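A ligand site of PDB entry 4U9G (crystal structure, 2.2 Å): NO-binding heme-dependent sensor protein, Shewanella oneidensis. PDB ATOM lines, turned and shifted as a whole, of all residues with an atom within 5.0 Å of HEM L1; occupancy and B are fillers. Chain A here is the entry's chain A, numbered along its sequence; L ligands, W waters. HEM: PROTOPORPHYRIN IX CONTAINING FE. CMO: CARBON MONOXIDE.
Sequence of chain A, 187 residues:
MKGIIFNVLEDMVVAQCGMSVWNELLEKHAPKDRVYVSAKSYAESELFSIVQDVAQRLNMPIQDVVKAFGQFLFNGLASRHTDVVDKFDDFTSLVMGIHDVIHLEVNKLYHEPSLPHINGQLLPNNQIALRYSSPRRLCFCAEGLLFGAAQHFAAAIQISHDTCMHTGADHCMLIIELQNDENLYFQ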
ATOM      1  N   MET A   1     -23.678  28.921  22.723  1.00  0.00           N
ATOM      2  CA  MET A   1     -24.143  27.531  22.484  1.00  0.00           C
ATOM      3  C   MET A   1     -22.964  26.563  22.482  1.00  0.00           C
ATOM      4  O   MET A   1     -22.053  26.678  21.643  1.00  0.00           O
ATOM      5  CB  MET A   1     -24.913  27.442  21.169  1.00  0.00           C
ATOM      6  CG  MET A   1     -25.646  26.120  20.954  1.00  0.00           C
ATOM      7  SD  MET A   1     -27.058  25.887  22.047  1.00  0.00           S
ATOM      8  CE  MET A   1     -28.138  27.199  21.498  1.00  0.00           C
ATOM      9  N   LYS A   2     -22.974  25.613  23.408  1.00  0.00           N
ATOM     10  CA  LYS A   2     -21.845  24.708  23.571  1.00  0.00           C
ATOM     11  C   LYS A   2     -21.722  23.705  22.435  1.00  0.00           C
ATOM     12  O   LYS A   2     -22.726  23.252  21.875  1.00  0.00           O
ATOM     13  CB  LYS A   2     -21.930  23.967  24.909  1.00  0.00           C
ATOM     14  CG  LYS A   2     -21.685  24.847  26.134  1.00  0.00           C
ATOM     15  CD  LYS A   2     -20.309  25.489  26.099  1.00  0.00           C
ATOM     16  CE  LYS A   2     -20.046  26.336  27.323  1.00  0.00           C
ATOM     17  NZ  LYS A   2     -18.702  26.966  27.265  1.00  0.00           N
ATOM     18  N   ILE A   4     -21.154  20.656  22.353  1.00  0.00           N
ATOM     19  CA  ILE A   4     -21.834  19.380  22.569  1.00  0.00           C
ATOM     20  C   ILE A   4     -23.206  19.358  21.918  1.00  0.00           C
ATOM     21  O   ILE A   4     -23.639  18.322  21.417  1.00  0.00           O
ATOM     22  CB  ILE A   4     -21.987  19.051  24.065  1.00  0.00           C
ATOM     23  CG1 ILE A   4     -22.646  17.683  24.199  1.00  0.00           C
ATOM     24  CG2 ILE A   4     -22.813  20.117  24.785  1.00  0.00           C
ATOM     25  CD1 ILE A   4     -22.536  17.086  25.550  1.00  0.00           C
ATOM     26  N   ILE A   5     -23.894  20.498  21.927  1.00  0.00           N
ATOM     27  CA  ILE A   5     -25.213  20.571  21.310  1.00  0.00           C
ATOM     28  C   ILE A   5     -25.070  20.376  19.800  1.00  0.00           C
ATOM     29  O   ILE A   5     -25.833  19.623  19.196  1.00  0.00           O
ATOM     30  CB  ILE A   5     -25.913  21.920  21.607  1.00  0.00           C
ATOM     31  CG1 ILE A   5     -25.982  22.181  23.113  1.00  0.00           C
ATOM     32  CG2 ILE A   5     -27.319  21.927  21.022  1.00  0.00           C
ATOM     33  CD1 ILE A   5     -26.641  21.082  23.927  1.00  0.00           C
ATOM     34  N   PHE A  74     -31.848  14.476  24.415  1.00  0.00           N
ATOM     35  CA  PHE A  74     -31.792  13.986  25.788  1.00  0.00           C
ATOM     36  C   PHE A  74     -30.938  12.728  25.869  1.00  0.00           C
ATOM     37  O   PHE A  74     -30.158  12.570  26.814  1.00  0.00           O
ATOM     38  CB  PHE A  74     -33.170  13.671  26.366  1.00  0.00           C
ATOM     39  CG  PHE A  74     -33.100  13.217  27.790  1.00  0.00           C
ATOM     40  CD1 PHE A  74     -32.877  11.880  28.101  1.00  0.00           C
ATOM     41  CD2 PHE A  74     -33.206  14.132  28.829  1.00  0.00           C
ATOM     42  CE1 PHE A  74     -32.770  11.465  29.417  1.00  0.00           C
ATOM     43  CE2 PHE A  74     -33.109  13.715  30.142  1.00  0.00           C
ATOM     44  CZ  PHE A  74     -32.891  12.381  30.436  1.00  0.00           C
ATOM     45  N   LEU A  77     -27.196  13.493  25.562  1.00  0.00           N
ATOM     46  CA  LEU A  77     -26.619  14.019  26.788  1.00  0.00           C
ATOM     47  C   LEU A  77     -26.577  13.017  27.909  1.00  0.00           C
ATOM     48  O   LEU A  77     -25.630  13.010  28.693  1.00  0.00           O
ATOM     49  CB  LEU A  77     -27.403  15.222  27.228  1.00  0.00           C
ATOM     50  CG  LEU A  77     -27.188  16.323  26.208  1.00  0.00           C
ATOM     51  CD1 LEU A  77     -28.246  17.222  26.460  1.00  0.00           C
ATOM     52  CD2 LEU A  77     -25.887  17.051  26.387  1.00  0.00           C
ATOM     53  N   HIS A  81     -23.245  12.368  29.654  1.00  0.00           N
ATOM     54  CA  HIS A  81     -23.210  12.707  31.083  1.00  0.00           C
ATOM     55  C   HIS A  81     -24.010  11.710  31.887  1.00  0.00           C
ATOM     56  O   HIS A  81     -24.951  12.073  32.595  1.00  0.00           O
ATOM     57  CB  HIS A  81     -23.752  14.118  31.313  1.00  0.00           C
ATOM     58  CG  HIS A  81     -22.948  15.199  30.666  1.00  0.00           C
ATOM     59  ND1 HIS A  81     -21.666  15.516  31.055  1.00  0.00           N
ATOM     60  CD2 HIS A  81     -23.249  16.031  29.645  1.00  0.00           C
ATOM     61  CE1 HIS A  81     -21.208  16.498  30.311  1.00  0.00           C
ATOM     62  NE2 HIS A  81     -22.149  16.831  29.446  1.00  0.00           N
ATOM     63  N   VAL A  84     -24.606  12.236  35.629  1.00  0.00           N
ATOM     64  CA  VAL A  84     -25.577  13.260  36.004  1.00  0.00           C
ATOM     65  C   VAL A  84     -27.000  12.680  36.010  1.00  0.00           C
ATOM     66  O   VAL A  84     -27.751  12.858  36.971  1.00  0.00           O
ATOM     67  CB  VAL A  84     -25.541  14.477  35.057  1.00  0.00           C
ATOM     68  CG1 VAL A  84     -26.610  15.498  35.431  1.00  0.00           C
ATOM     69  CG2 VAL A  84     -24.167  15.133  35.101  1.00  0.00           C
ATOM     70  N   VAL A  85     -27.349  11.980  34.943  1.00  0.00           N
ATOM     71  CA  VAL A  85     -28.697  11.435  34.804  1.00  0.00           C
ATOM     72  C   VAL A  85     -28.944  10.258  35.756  1.00  0.00           C
ATOM     73  O   VAL A  85     -30.072  10.038  36.190  1.00  0.00           O
ATOM     74  CB  VAL A  85     -28.973  10.996  33.343  1.00  0.00           C
ATOM     75  CG1 VAL A  85     -30.328  10.303  33.193  1.00  0.00           C
ATOM     76  CG2 VAL A  85     -28.901  12.213  32.416  1.00  0.00           C
ATOM     77  N   LEU A  94     -36.212  13.542  38.056  1.00  0.00           N
ATOM     78  CA  LEU A  94     -35.298  14.193  37.137  1.00  0.00           C
ATOM     79  C   LEU A  94     -35.815  15.570  36.741  1.00  0.00           C
ATOM     80  O   LEU A  94     -35.057  16.539  36.715  1.00  0.00           O
ATOM     81  CB  LEU A  94     -35.078  13.343  35.873  1.00  0.00           C
ATOM     82  CG  LEU A  94     -34.072  13.954  34.887  1.00  0.00           C
ATOM     83  CD1 LEU A  94     -33.226  12.883  34.227  1.00  0.00           C
ATOM     84  CD2 LEU A  94     -34.777  14.806  33.817  1.00  0.00           C
ATOM     85  N   ILE A  98     -33.979  19.376  37.257  1.00  0.00           N
ATOM     86  CA  ILE A  98     -33.349  19.935  36.062  1.00  0.00           C
ATOM     87  C   ILE A  98     -32.539  21.173  36.403  1.00  0.00           C
ATOM     88  O   ILE A  98     -31.387  21.320  35.977  1.00  0.00           O
ATOM     89  CB  ILE A  98     -34.378  20.312  34.988  1.00  0.00           C
ATOM     90  CG1 ILE A  98     -35.074  19.058  34.460  1.00  0.00           C
ATOM     91  CG2 ILE A  98     -33.698  21.048  33.814  1.00  0.00           C
ATOM     92  CD1 ILE A  98     -36.334  19.357  33.663  1.00  0.00           C
ATOM     93  N   ILE A 102     -29.165  19.139  37.647  1.00  0.00           N
ATOM     94  CA  ILE A 102     -28.599  18.887  36.321  1.00  0.00           C
ATOM     95  C   ILE A 102     -27.888  20.127  35.786  1.00  0.00           C
ATOM     96  O   ILE A 102     -26.682  20.104  35.560  1.00  0.00           O
ATOM     97  CB  ILE A 102     -29.702  18.442  35.331  1.00  0.00           C
ATOM     98  CG1 ILE A 102     -30.289  17.111  35.802  1.00  0.00           C
ATOM     99  CG2 ILE A 102     -29.136  18.304  33.918  1.00  0.00           C
ATOM    100  CD1 ILE A 102     -31.399  16.550  34.945  1.00  0.00           C
ATOM    101  N   HIS A 103     -28.628  21.209  35.576  1.00  0.00           N
ATOM    102  CA  HIS A 103     -28.029  22.410  35.013  1.00  0.00           C
ATOM    103  C   HIS A 103     -27.077  23.082  36.005  1.00  0.00           C
ATOM    104  O   HIS A 103     -26.166  23.817  35.604  1.00  0.00           O
ATOM    105  CB  HIS A 103     -29.124  23.375  34.550  1.00  0.00           C
ATOM    106  CG  HIS A 103     -29.754  22.988  33.247  1.00  0.00           C
ATOM    107  ND1 HIS A 103     -30.945  23.515  32.796  1.00  0.00           N
ATOM    108  CD2 HIS A 103     -29.355  22.105  32.285  1.00  0.00           C
ATOM    109  CE1 HIS A 103     -31.246  22.990  31.627  1.00  0.00           C
ATOM    110  NE2 HIS A 103     -30.308  22.129  31.297  1.00  0.00           N
ATOM    111  N   VAL A 106     -23.998  21.423  35.212  1.00  0.00           N
ATOM    112  CA  VAL A 106     -23.527  21.887  33.917  1.00  0.00           C
ATOM    113  C   VAL A 106     -22.655  23.134  34.079  1.00  0.00           C
ATOM    114  O   VAL A 106     -21.744  23.359  33.288  1.00  0.00           O
ATOM    115  CB  VAL A 106     -24.716  22.152  32.967  1.00  0.00           C
ATOM    116  CG1 VAL A 106     -24.279  22.870  31.699  1.00  0.00           C
ATOM    117  CG2 VAL A 106     -25.392  20.852  32.603  1.00  0.00           C
ATOM    118  N   TYR A 110     -18.964  22.856  32.516  1.00  0.00           N
ATOM    119  CA  TYR A 110     -18.705  23.755  31.391  1.00  0.00           C
ATOM    120  C   TYR A 110     -18.395  25.177  31.851  1.00  0.00           C
ATOM    121  O   TYR A 110     -18.948  25.650  32.843  1.00  0.00           O
ATOM    122  CB  TYR A 110     -19.908  23.788  30.440  1.00  0.00           C
ATOM    123  CG  TYR A 110     -20.218  22.484  29.758  1.00  0.00           C
ATOM    124  CD1 TYR A 110     -21.053  21.543  30.350  1.00  0.00           C
ATOM    125  CD2 TYR A 110     -19.685  22.189  28.507  1.00  0.00           C
ATOM    126  CE1 TYR A 110     -21.331  20.333  29.728  1.00  0.00           C
ATOM    127  CE2 TYR A 110     -19.964  20.998  27.875  1.00  0.00           C
ATOM    128  CZ  TYR A 110     -20.780  20.070  28.496  1.00  0.00           C
ATOM    129  OH  TYR A 110     -21.041  18.882  27.848  1.00  0.00           O
ATOM    130  N   GLU A 112     -19.013  28.837  31.804  1.00  0.00           N
ATOM    131  CA  GLU A 112     -20.067  29.812  31.504  1.00  0.00           C
ATOM    132  C   GLU A 112     -21.056  29.374  30.425  1.00  0.00           C
ATOM    133  O   GLU A 112     -21.140  29.978  29.350  1.00  0.00           O
ATOM    134  CB  GLU A 112     -19.425  31.138  31.088  1.00  0.00           C
ATOM    135  CG  GLU A 112     -18.625  31.791  32.216  1.00  0.00           C
ATOM    136  CD  GLU A 112     -17.907  33.056  31.782  1.00  0.00           C
ATOM    137  OE1 GLU A 112     -18.129  33.506  30.645  1.00  0.00           O
ATOM    138  OE2 GLU A 112     -17.124  33.594  32.589  1.00  0.00           O
ATOM    139  N   PRO A 113     -21.831  28.320  30.722  1.00  0.00           N
ATOM    140  CA  PRO A 113     -22.865  27.859  29.788  1.00  0.00           C
ATOM    141  C   PRO A 113     -24.024  28.853  29.703  1.00  0.00           C
ATOM    142  O   PRO A 113     -24.187  29.655  30.618  1.00  0.00           O
ATOM    143  CB  PRO A 113     -23.321  26.538  30.418  1.00  0.00           C
ATOM    144  CG  PRO A 113     -23.135  26.769  31.888  1.00  0.00           C
ATOM    145  CD  PRO A 113     -21.864  27.572  31.994  1.00  0.00           C
ATOM    146  N   SER A 114     -24.796  28.792  28.617  1.00  0.00           N
ATOM    147  CA  SER A 114     -25.973  29.635  28.469  1.00  0.00           C
ATOM    148  C   SER A 114     -27.216  28.785  28.640  1.00  0.00           C
ATOM    149  O   SER A 114     -27.632  28.071  27.738  1.00  0.00           O
ATOM    150  CB  SER A 114     -25.960  30.342  27.108  1.00  0.00           C
ATOM    151  OG  SER A 114     -24.987  31.367  27.095  1.00  0.00           O
ATOM    152  N   LEU A 115     -27.802  28.876  29.834  1.00  0.00           N
ATOM    153  CA  LEU A 115     -28.830  27.955  30.269  1.00  0.00           C
ATOM    154  C   LEU A 115     -30.162  28.656  30.516  1.00  0.00           C
ATOM    155  O   LEU A 115     -30.184  29.848  30.834  1.00  0.00           O
ATOM    156  CB  LEU A 115     -28.375  27.246  31.546  1.00  0.00           C
ATOM    157  CG  LEU A 115     -27.229  26.243  31.374  1.00  0.00           C
ATOM    158  CD1 LEU A 115     -26.586  25.919  32.709  1.00  0.00           C
ATOM    159  CD2 LEU A 115     -27.727  24.981  30.697  1.00  0.00           C
ATOM    160  N   PRO A 116     -31.283  27.932  30.379  1.00  0.00           N
ATOM    161  CA  PRO A 116     -32.571  28.537  30.679  1.00  0.00           C
ATOM    162  C   PRO A 116     -32.763  28.680  32.174  1.00  0.00           C
ATOM    163  O   PRO A 116     -31.983  28.118  32.936  1.00  0.00           O
ATOM    164  CB  PRO A 116     -33.568  27.554  30.092  1.00  0.00           C
ATOM    165  CG  PRO A 116     -32.897  26.229  30.278  1.00  0.00           C
ATOM    166  CD  PRO A 116     -31.418  26.495  30.065  1.00  0.00           C
ATOM    167  N   ILE A 118     -35.392  27.485  34.917  1.00  0.00           N
ATOM    168  CA  ILE A 118     -36.451  26.505  35.036  1.00  0.00           C
ATOM    169  C   ILE A 118     -36.854  26.308  36.501  1.00  0.00           C
ATOM    170  O   ILE A 118     -36.012  26.333  37.385  1.00  0.00           O
ATOM    171  CB  ILE A 118     -36.025  25.154  34.417  1.00  0.00           C
ATOM    172  CG1 ILE A 118     -35.941  25.303  32.893  1.00  0.00           C
ATOM    173  CG2 ILE A 118     -37.003  24.037  34.783  1.00  0.00           C
ATOM    174  CD1 ILE A 118     -35.458  24.074  32.152  1.00  0.00           C
ATOM    175  N   LEU A 130     -43.993  22.912  34.902  1.00  0.00           N
ATOM    176  CA  LEU A 130     -42.631  23.331  34.621  1.00  0.00           C
ATOM    177  C   LEU A 130     -42.619  24.713  33.964  1.00  0.00           C
ATOM    178  O   LEU A 130     -43.078  24.873  32.833  1.00  0.00           O
ATOM    179  CB  LEU A 130     -41.909  22.304  33.732  1.00  0.00           C
ATOM    180  CG  LEU A 130     -40.384  22.389  33.744  1.00  0.00           C
ATOM    181  CD1 LEU A 130     -39.833  21.949  35.096  1.00  0.00           C
ATOM    182  CD2 LEU A 130     -39.784  21.541  32.628  1.00  0.00           C
ATOM    183  N   TYR A 132     -40.643  27.734  32.286  1.00  0.00           N
ATOM    184  CA  TYR A 132     -39.427  27.916  31.502  1.00  0.00           C
ATOM    185  C   TYR A 132     -39.243  29.361  31.088  1.00  0.00           C
ATOM    186  O   TYR A 132     -40.205  30.045  30.722  1.00  0.00           O
ATOM    187  CB  TYR A 132     -39.460  26.997  30.272  1.00  0.00           C
ATOM    188  CG  TYR A 132     -38.412  27.311  29.210  1.00  0.00           C
ATOM    189  CD1 TYR A 132     -38.636  28.301  28.266  1.00  0.00           C
ATOM    190  CD2 TYR A 132     -37.221  26.611  29.144  1.00  0.00           C
ATOM    191  CE1 TYR A 132     -37.691  28.601  27.302  1.00  0.00           C
ATOM    192  CE2 TYR A 132     -36.272  26.890  28.179  1.00  0.00           C
ATOM    193  CZ  TYR A 132     -36.518  27.889  27.257  1.00  0.00           C
ATOM    194  OH  TYR A 132     -35.586  28.182  26.301  1.00  0.00           O
ATOM    195  N   SER A 134     -36.148  31.917  29.045  1.00  0.00           N
ATOM    196  CA  SER A 134     -34.846  32.074  28.414  1.00  0.00           C
ATOM    197  C   SER A 134     -34.930  33.053  27.246  1.00  0.00           C
ATOM    198  O   SER A 134     -35.915  33.057  26.505  1.00  0.00           O
ATOM    199  CB  SER A 134     -34.327  30.734  27.911  1.00  0.00           C
ATOM    200  OG  SER A 134     -33.201  30.896  27.065  1.00  0.00           O
ATOM    201  N   ARG A 136     -33.381  32.815  24.618  1.00  0.00           N
ATOM    202  CA  ARG A 136     -33.241  32.021  23.410  1.00  0.00           C
ATOM    203  C   ARG A 136     -34.574  31.409  22.981  1.00  0.00           C
ATOM    204  O   ARG A 136     -34.743  30.996  21.831  1.00  0.00           O
ATOM    205  CB  ARG A 136     -32.179  30.928  23.621  1.00  0.00           C
ATOM    206  CG  ARG A 136     -30.763  31.488  23.668  1.00  0.00           C
ATOM    207  CD  ARG A 136     -29.765  30.534  24.330  1.00  0.00           C
ATOM    208  NE  ARG A 136     -29.964  30.419  25.767  1.00  0.00           N
ATOM    209  CZ  ARG A 136     -29.579  31.337  26.660  1.00  0.00           C
ATOM    210  NH1 ARG A 136     -28.987  32.460  26.261  1.00  0.00           N
ATOM    211  NH2 ARG A 136     -29.799  31.143  27.951  1.00  0.00           N
ATOM    212  N   LEU A 138     -36.268  28.579  23.618  1.00  0.00           N
ATOM    213  CA  LEU A 138     -36.174  27.214  23.112  1.00  0.00           C
ATOM    214  C   LEU A 138     -37.102  26.280  23.870  1.00  0.00           C
ATOM    215  O   LEU A 138     -36.739  25.138  24.166  1.00  0.00           O
ATOM    216  CB  LEU A 138     -34.727  26.732  23.190  1.00  0.00           C
ATOM    217  CG  LEU A 138     -33.789  27.416  22.197  1.00  0.00           C
ATOM    218  CD1 LEU A 138     -32.329  27.158  22.546  1.00  0.00           C
ATOM    219  CD2 LEU A 138     -34.073  26.930  20.777  1.00  0.00           C
ATOM    220  N   CYS A 141     -37.616  22.926  22.360  1.00  0.00           N
ATOM    221  CA  CYS A 141     -36.511  22.026  22.605  1.00  0.00           C
ATOM    222  C   CYS A 141     -36.727  21.380  23.968  1.00  0.00           C
ATOM    223  O   CYS A 141     -36.524  20.180  24.122  1.00  0.00           O
ATOM    224  CB  CYS A 141     -35.159  22.741  22.563  1.00  0.00           C
ATOM    225  SG  CYS A 141     -33.735  21.609  22.617  1.00  0.00           S
ATOM    226  N   ALA A 142     -37.183  22.172  24.929  1.00  0.00           N
ATOM    227  CA  ALA A 142     -37.455  21.688  26.287  1.00  0.00           C
ATOM    228  C   ALA A 142     -38.521  20.601  26.267  1.00  0.00           C
ATOM    229  O   ALA A 142     -38.389  19.593  26.965  1.00  0.00           O
ATOM    230  CB  ALA A 142     -37.882  22.834  27.202  1.00  0.00           C
ATOM    231  N   LEU A 145     -36.995  17.401  24.981  1.00  0.00           N
ATOM    232  CA  LEU A 145     -36.152  16.836  26.019  1.00  0.00           C
ATOM    233  C   LEU A 145     -36.944  16.102  27.086  1.00  0.00           C
ATOM    234  O   LEU A 145     -36.523  15.048  27.567  1.00  0.00           O
ATOM    235  CB  LEU A 145     -35.326  17.937  26.659  1.00  0.00           C
ATOM    236  CG  LEU A 145     -34.216  18.324  25.704  1.00  0.00           C
ATOM    237  CD1 LEU A 145     -34.002  19.810  25.856  1.00  0.00           C
ATOM    238  CD2 LEU A 145     -32.985  17.480  26.014  1.00  0.00           C
ATOM    239  N   LEU A 146     -38.081  16.664  27.471  1.00  0.00           N
ATOM    240  CA  LEU A 146     -38.936  16.031  28.448  1.00  0.00           C
ATOM    241  C   LEU A 146     -39.465  14.707  27.904  1.00  0.00           C
ATOM    242  O   LEU A 146     -39.565  13.731  28.637  1.00  0.00           O
ATOM    243  CB  LEU A 146     -40.088  16.946  28.838  1.00  0.00           C
ATOM    244  CG  LEU A 146     -39.674  18.172  29.656  1.00  0.00           C
ATOM    245  CD1 LEU A 146     -40.789  19.199  29.688  1.00  0.00           C
ATOM    246  CD2 LEU A 146     -39.282  17.770  31.078  1.00  0.00           C
ATOM    247  N   ALA A 149     -36.599  12.346  28.208  1.00  0.00           N
ATOM    248  CA  ALA A 149     -36.454  11.894  29.586  1.00  0.00           C
ATOM    249  C   ALA A 149     -37.501  10.831  29.929  1.00  0.00           C
ATOM    250  O   ALA A 149     -37.213   9.862  30.629  1.00  0.00           O
ATOM    251  CB  ALA A 149     -36.554  13.071  30.548  1.00  0.00           C
HETATM  252  CHA HEM L   1     -29.184  24.027  27.621  1.00  0.00           C
HETATM  253  CHB HEM L   1     -33.539  22.249  29.114  1.00  0.00           C
HETATM  254  CHC HEM L   1     -31.504  18.047  30.667  1.00  0.00           C
HETATM  255  CHD HEM L   1     -27.121  20.101  29.913  1.00  0.00           C
HETATM  256  C1A HEM L   1     -30.569  23.800  27.696  1.00  0.00           C
HETATM  257  C2A HEM L   1     -31.629  24.391  26.873  1.00  0.00           C
HETATM  258  C3A HEM L   1     -32.816  23.902  27.300  1.00  0.00           C
HETATM  259  C4A HEM L   1     -32.570  22.972  28.397  1.00  0.00           C
HETATM  260  CMA HEM L   1     -34.223  24.235  26.728  1.00  0.00           C
HETATM  261  CAA HEM L   1     -31.395  25.399  25.723  1.00  0.00           C
HETATM  262  CBA HEM L   1     -30.870  26.727  26.275  1.00  0.00           C
HETATM  263  CGA HEM L   1     -32.007  27.623  26.717  1.00  0.00           C
HETATM  264  O1A HEM L   1     -31.724  28.759  27.157  1.00  0.00           O
HETATM  265  O2A HEM L   1     -33.198  27.218  26.633  1.00  0.00           O
HETATM  266  C1B HEM L   1     -33.386  20.947  29.602  1.00  0.00           C
HETATM  267  C2B HEM L   1     -34.447  20.014  29.989  1.00  0.00           C
HETATM  268  C3B HEM L   1     -33.883  18.863  30.418  1.00  0.00           C
HETATM  269  C4B HEM L   1     -32.448  19.014  30.318  1.00  0.00           C
HETATM  270  CMB HEM L   1     -35.950  20.360  29.906  1.00  0.00           C
HETATM  271  CAB HEM L   1     -34.522  17.538  30.931  1.00  0.00           C
HETATM  272  CBB HEM L   1     -35.790  17.179  30.714  1.00  0.00           C
HETATM  273  C1C HEM L   1     -30.136  18.215  30.560  1.00  0.00           C
HETATM  274  C2C HEM L   1     -29.110  17.216  30.809  1.00  0.00           C
HETATM  275  C3C HEM L   1     -27.914  17.776  30.585  1.00  0.00           C
HETATM  276  C4C HEM L   1     -28.113  19.164  30.216  1.00  0.00           C
HETATM  277  CMC HEM L   1     -29.401  15.747  31.227  1.00  0.00           C
HETATM  278  CAC HEM L   1     -26.520  17.123  30.749  1.00  0.00           C
HETATM  279  CBC HEM L   1     -26.237  16.398  31.835  1.00  0.00           C
HETATM  280  C1D HEM L   1     -27.263  21.229  29.096  1.00  0.00           C
HETATM  281  C2D HEM L   1     -26.192  21.824  28.307  1.00  0.00           C
HETATM  282  C3D HEM L   1     -26.838  23.038  27.591  1.00  0.00           C
HETATM  283  C4D HEM L   1     -28.230  23.081  28.014  1.00  0.00           C
HETATM  284  CMD HEM L   1     -24.720  21.342  28.193  1.00  0.00           C
HETATM  285  CAD HEM L   1     -26.127  24.010  26.618  1.00  0.00           C
HETATM  286  CBD HEM L   1     -25.657  25.244  27.377  1.00  0.00           C
HETATM  287  CGD HEM L   1     -24.928  26.129  26.405  1.00  0.00           C
HETATM  288  O1D HEM L   1     -25.012  25.872  25.181  1.00  0.00           O
HETATM  289  O2D HEM L   1     -24.257  27.094  26.855  1.00  0.00           O
HETATM  290  NA  HEM L   1     -31.198  22.941  28.600  1.00  0.00           N
HETATM  291  NB  HEM L   1     -32.183  20.293  29.825  1.00  0.00           N
HETATM  292  NC  HEM L   1     -29.482  19.389  30.195  1.00  0.00           N
HETATM  293  ND  HEM L   1     -28.422  21.994  28.895  1.00  0.00           N
HETATM  294 FE   HEM L   1     -30.368  21.104  29.338  1.00  0.00          FE
HETATM  295  C   CMO L   2     -30.349  20.376  27.589  1.00  0.00           C
HETATM  296  O   CMO L   2     -30.393  19.963  26.431  1.00  0.00           O
HETATM  297  O   HOH W   1     -22.522  28.679  25.328  1.00  0.00           O
HETATM  298  O   HOH W   2     -27.465  27.923  25.300  1.00  0.00           O
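FE of HEM L1 is bound by NE2 of His 103.
The backbone NH (N) of Ser 114 lies within hydrogen-bond range of an oxygen (O2D) of HEM L1.
An oxygen (O2A) of HEM L1 is in hydrogen-bond range of the side-chain hydroxyl (OH) of Tyr 132, 2.6 Å away.
OG of Ser 134 is in hydrogen-bond range of O1A of HEM L1, at 2.6 Å.
The backbone NH (N) of Lys 2 sits at hydrogen-bond distance from an oxygen (O1D) of HEM L1.
The guanidinium group (NE) of Arg 136 lies within salt-bridge range of an oxygen (O1A) of HEM L1, at 2.8 Å.
N of His 103 lies within hydrogen-bond range of O of Ile 98.
The side-chain hydroxyl (OH) of Tyr 132 is in hydrogen-bond range of the backbone NH (N) of Leu 138, 2.8 Å away.
The side-chain hydroxyl of Ser 134 sits close to the backbone NH of Arg 136, 3.1 Å away.
NH2 of Arg 136 sits at hydrogen-bond distance from O of Leu 115 (3.2 Å).
The side-chain hydroxyl (OH) of Tyr 110 sits at hydrogen-bond distance from a ring nitrogen (NE2) of His 81, 2.8 Å away.
An oxygen (O1D) of HEM L1 sits close to the side-chain sulfur of Met 1, 3.7 Å away.
N of Pro 116 lies close to O1A of HEM L1, 3.4 Å away.
Merely in contact with HEM L1: Val 106, Ile 102, Leu 115, Pro 113, His 81, Leu 146, Leu 138, Ile 98, Val 84, Val 85, Tyr 110, Leu 145, Ala 142, Ile 5 and Leu 94.
Hydrophobic or aromatic side chains within 4 Å of HEM L1: Met 1, Ile 5, His 81, Val 84, Val 85, Leu 94, Ile 98, Ile 102, His 103, Val 106, Tyr 110, Pro 113, Leu 115, Pro 116, Tyr 132, Leu 138, Ala 142, Leu 145 and Leu 146.
Of the 31 residues printed, 23 come within 4 Å of HEM L1.
Water W1 lies within hydrogen-bond range of O2D of HEM L1 and N of Met 1.
Water W2 lies within hydrogen-bond range of the backbone carbonyl oxygen (O) of Ser 114 (2.4 Å) and an oxygen (O1D) of HEM L1 (3.2 Å).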
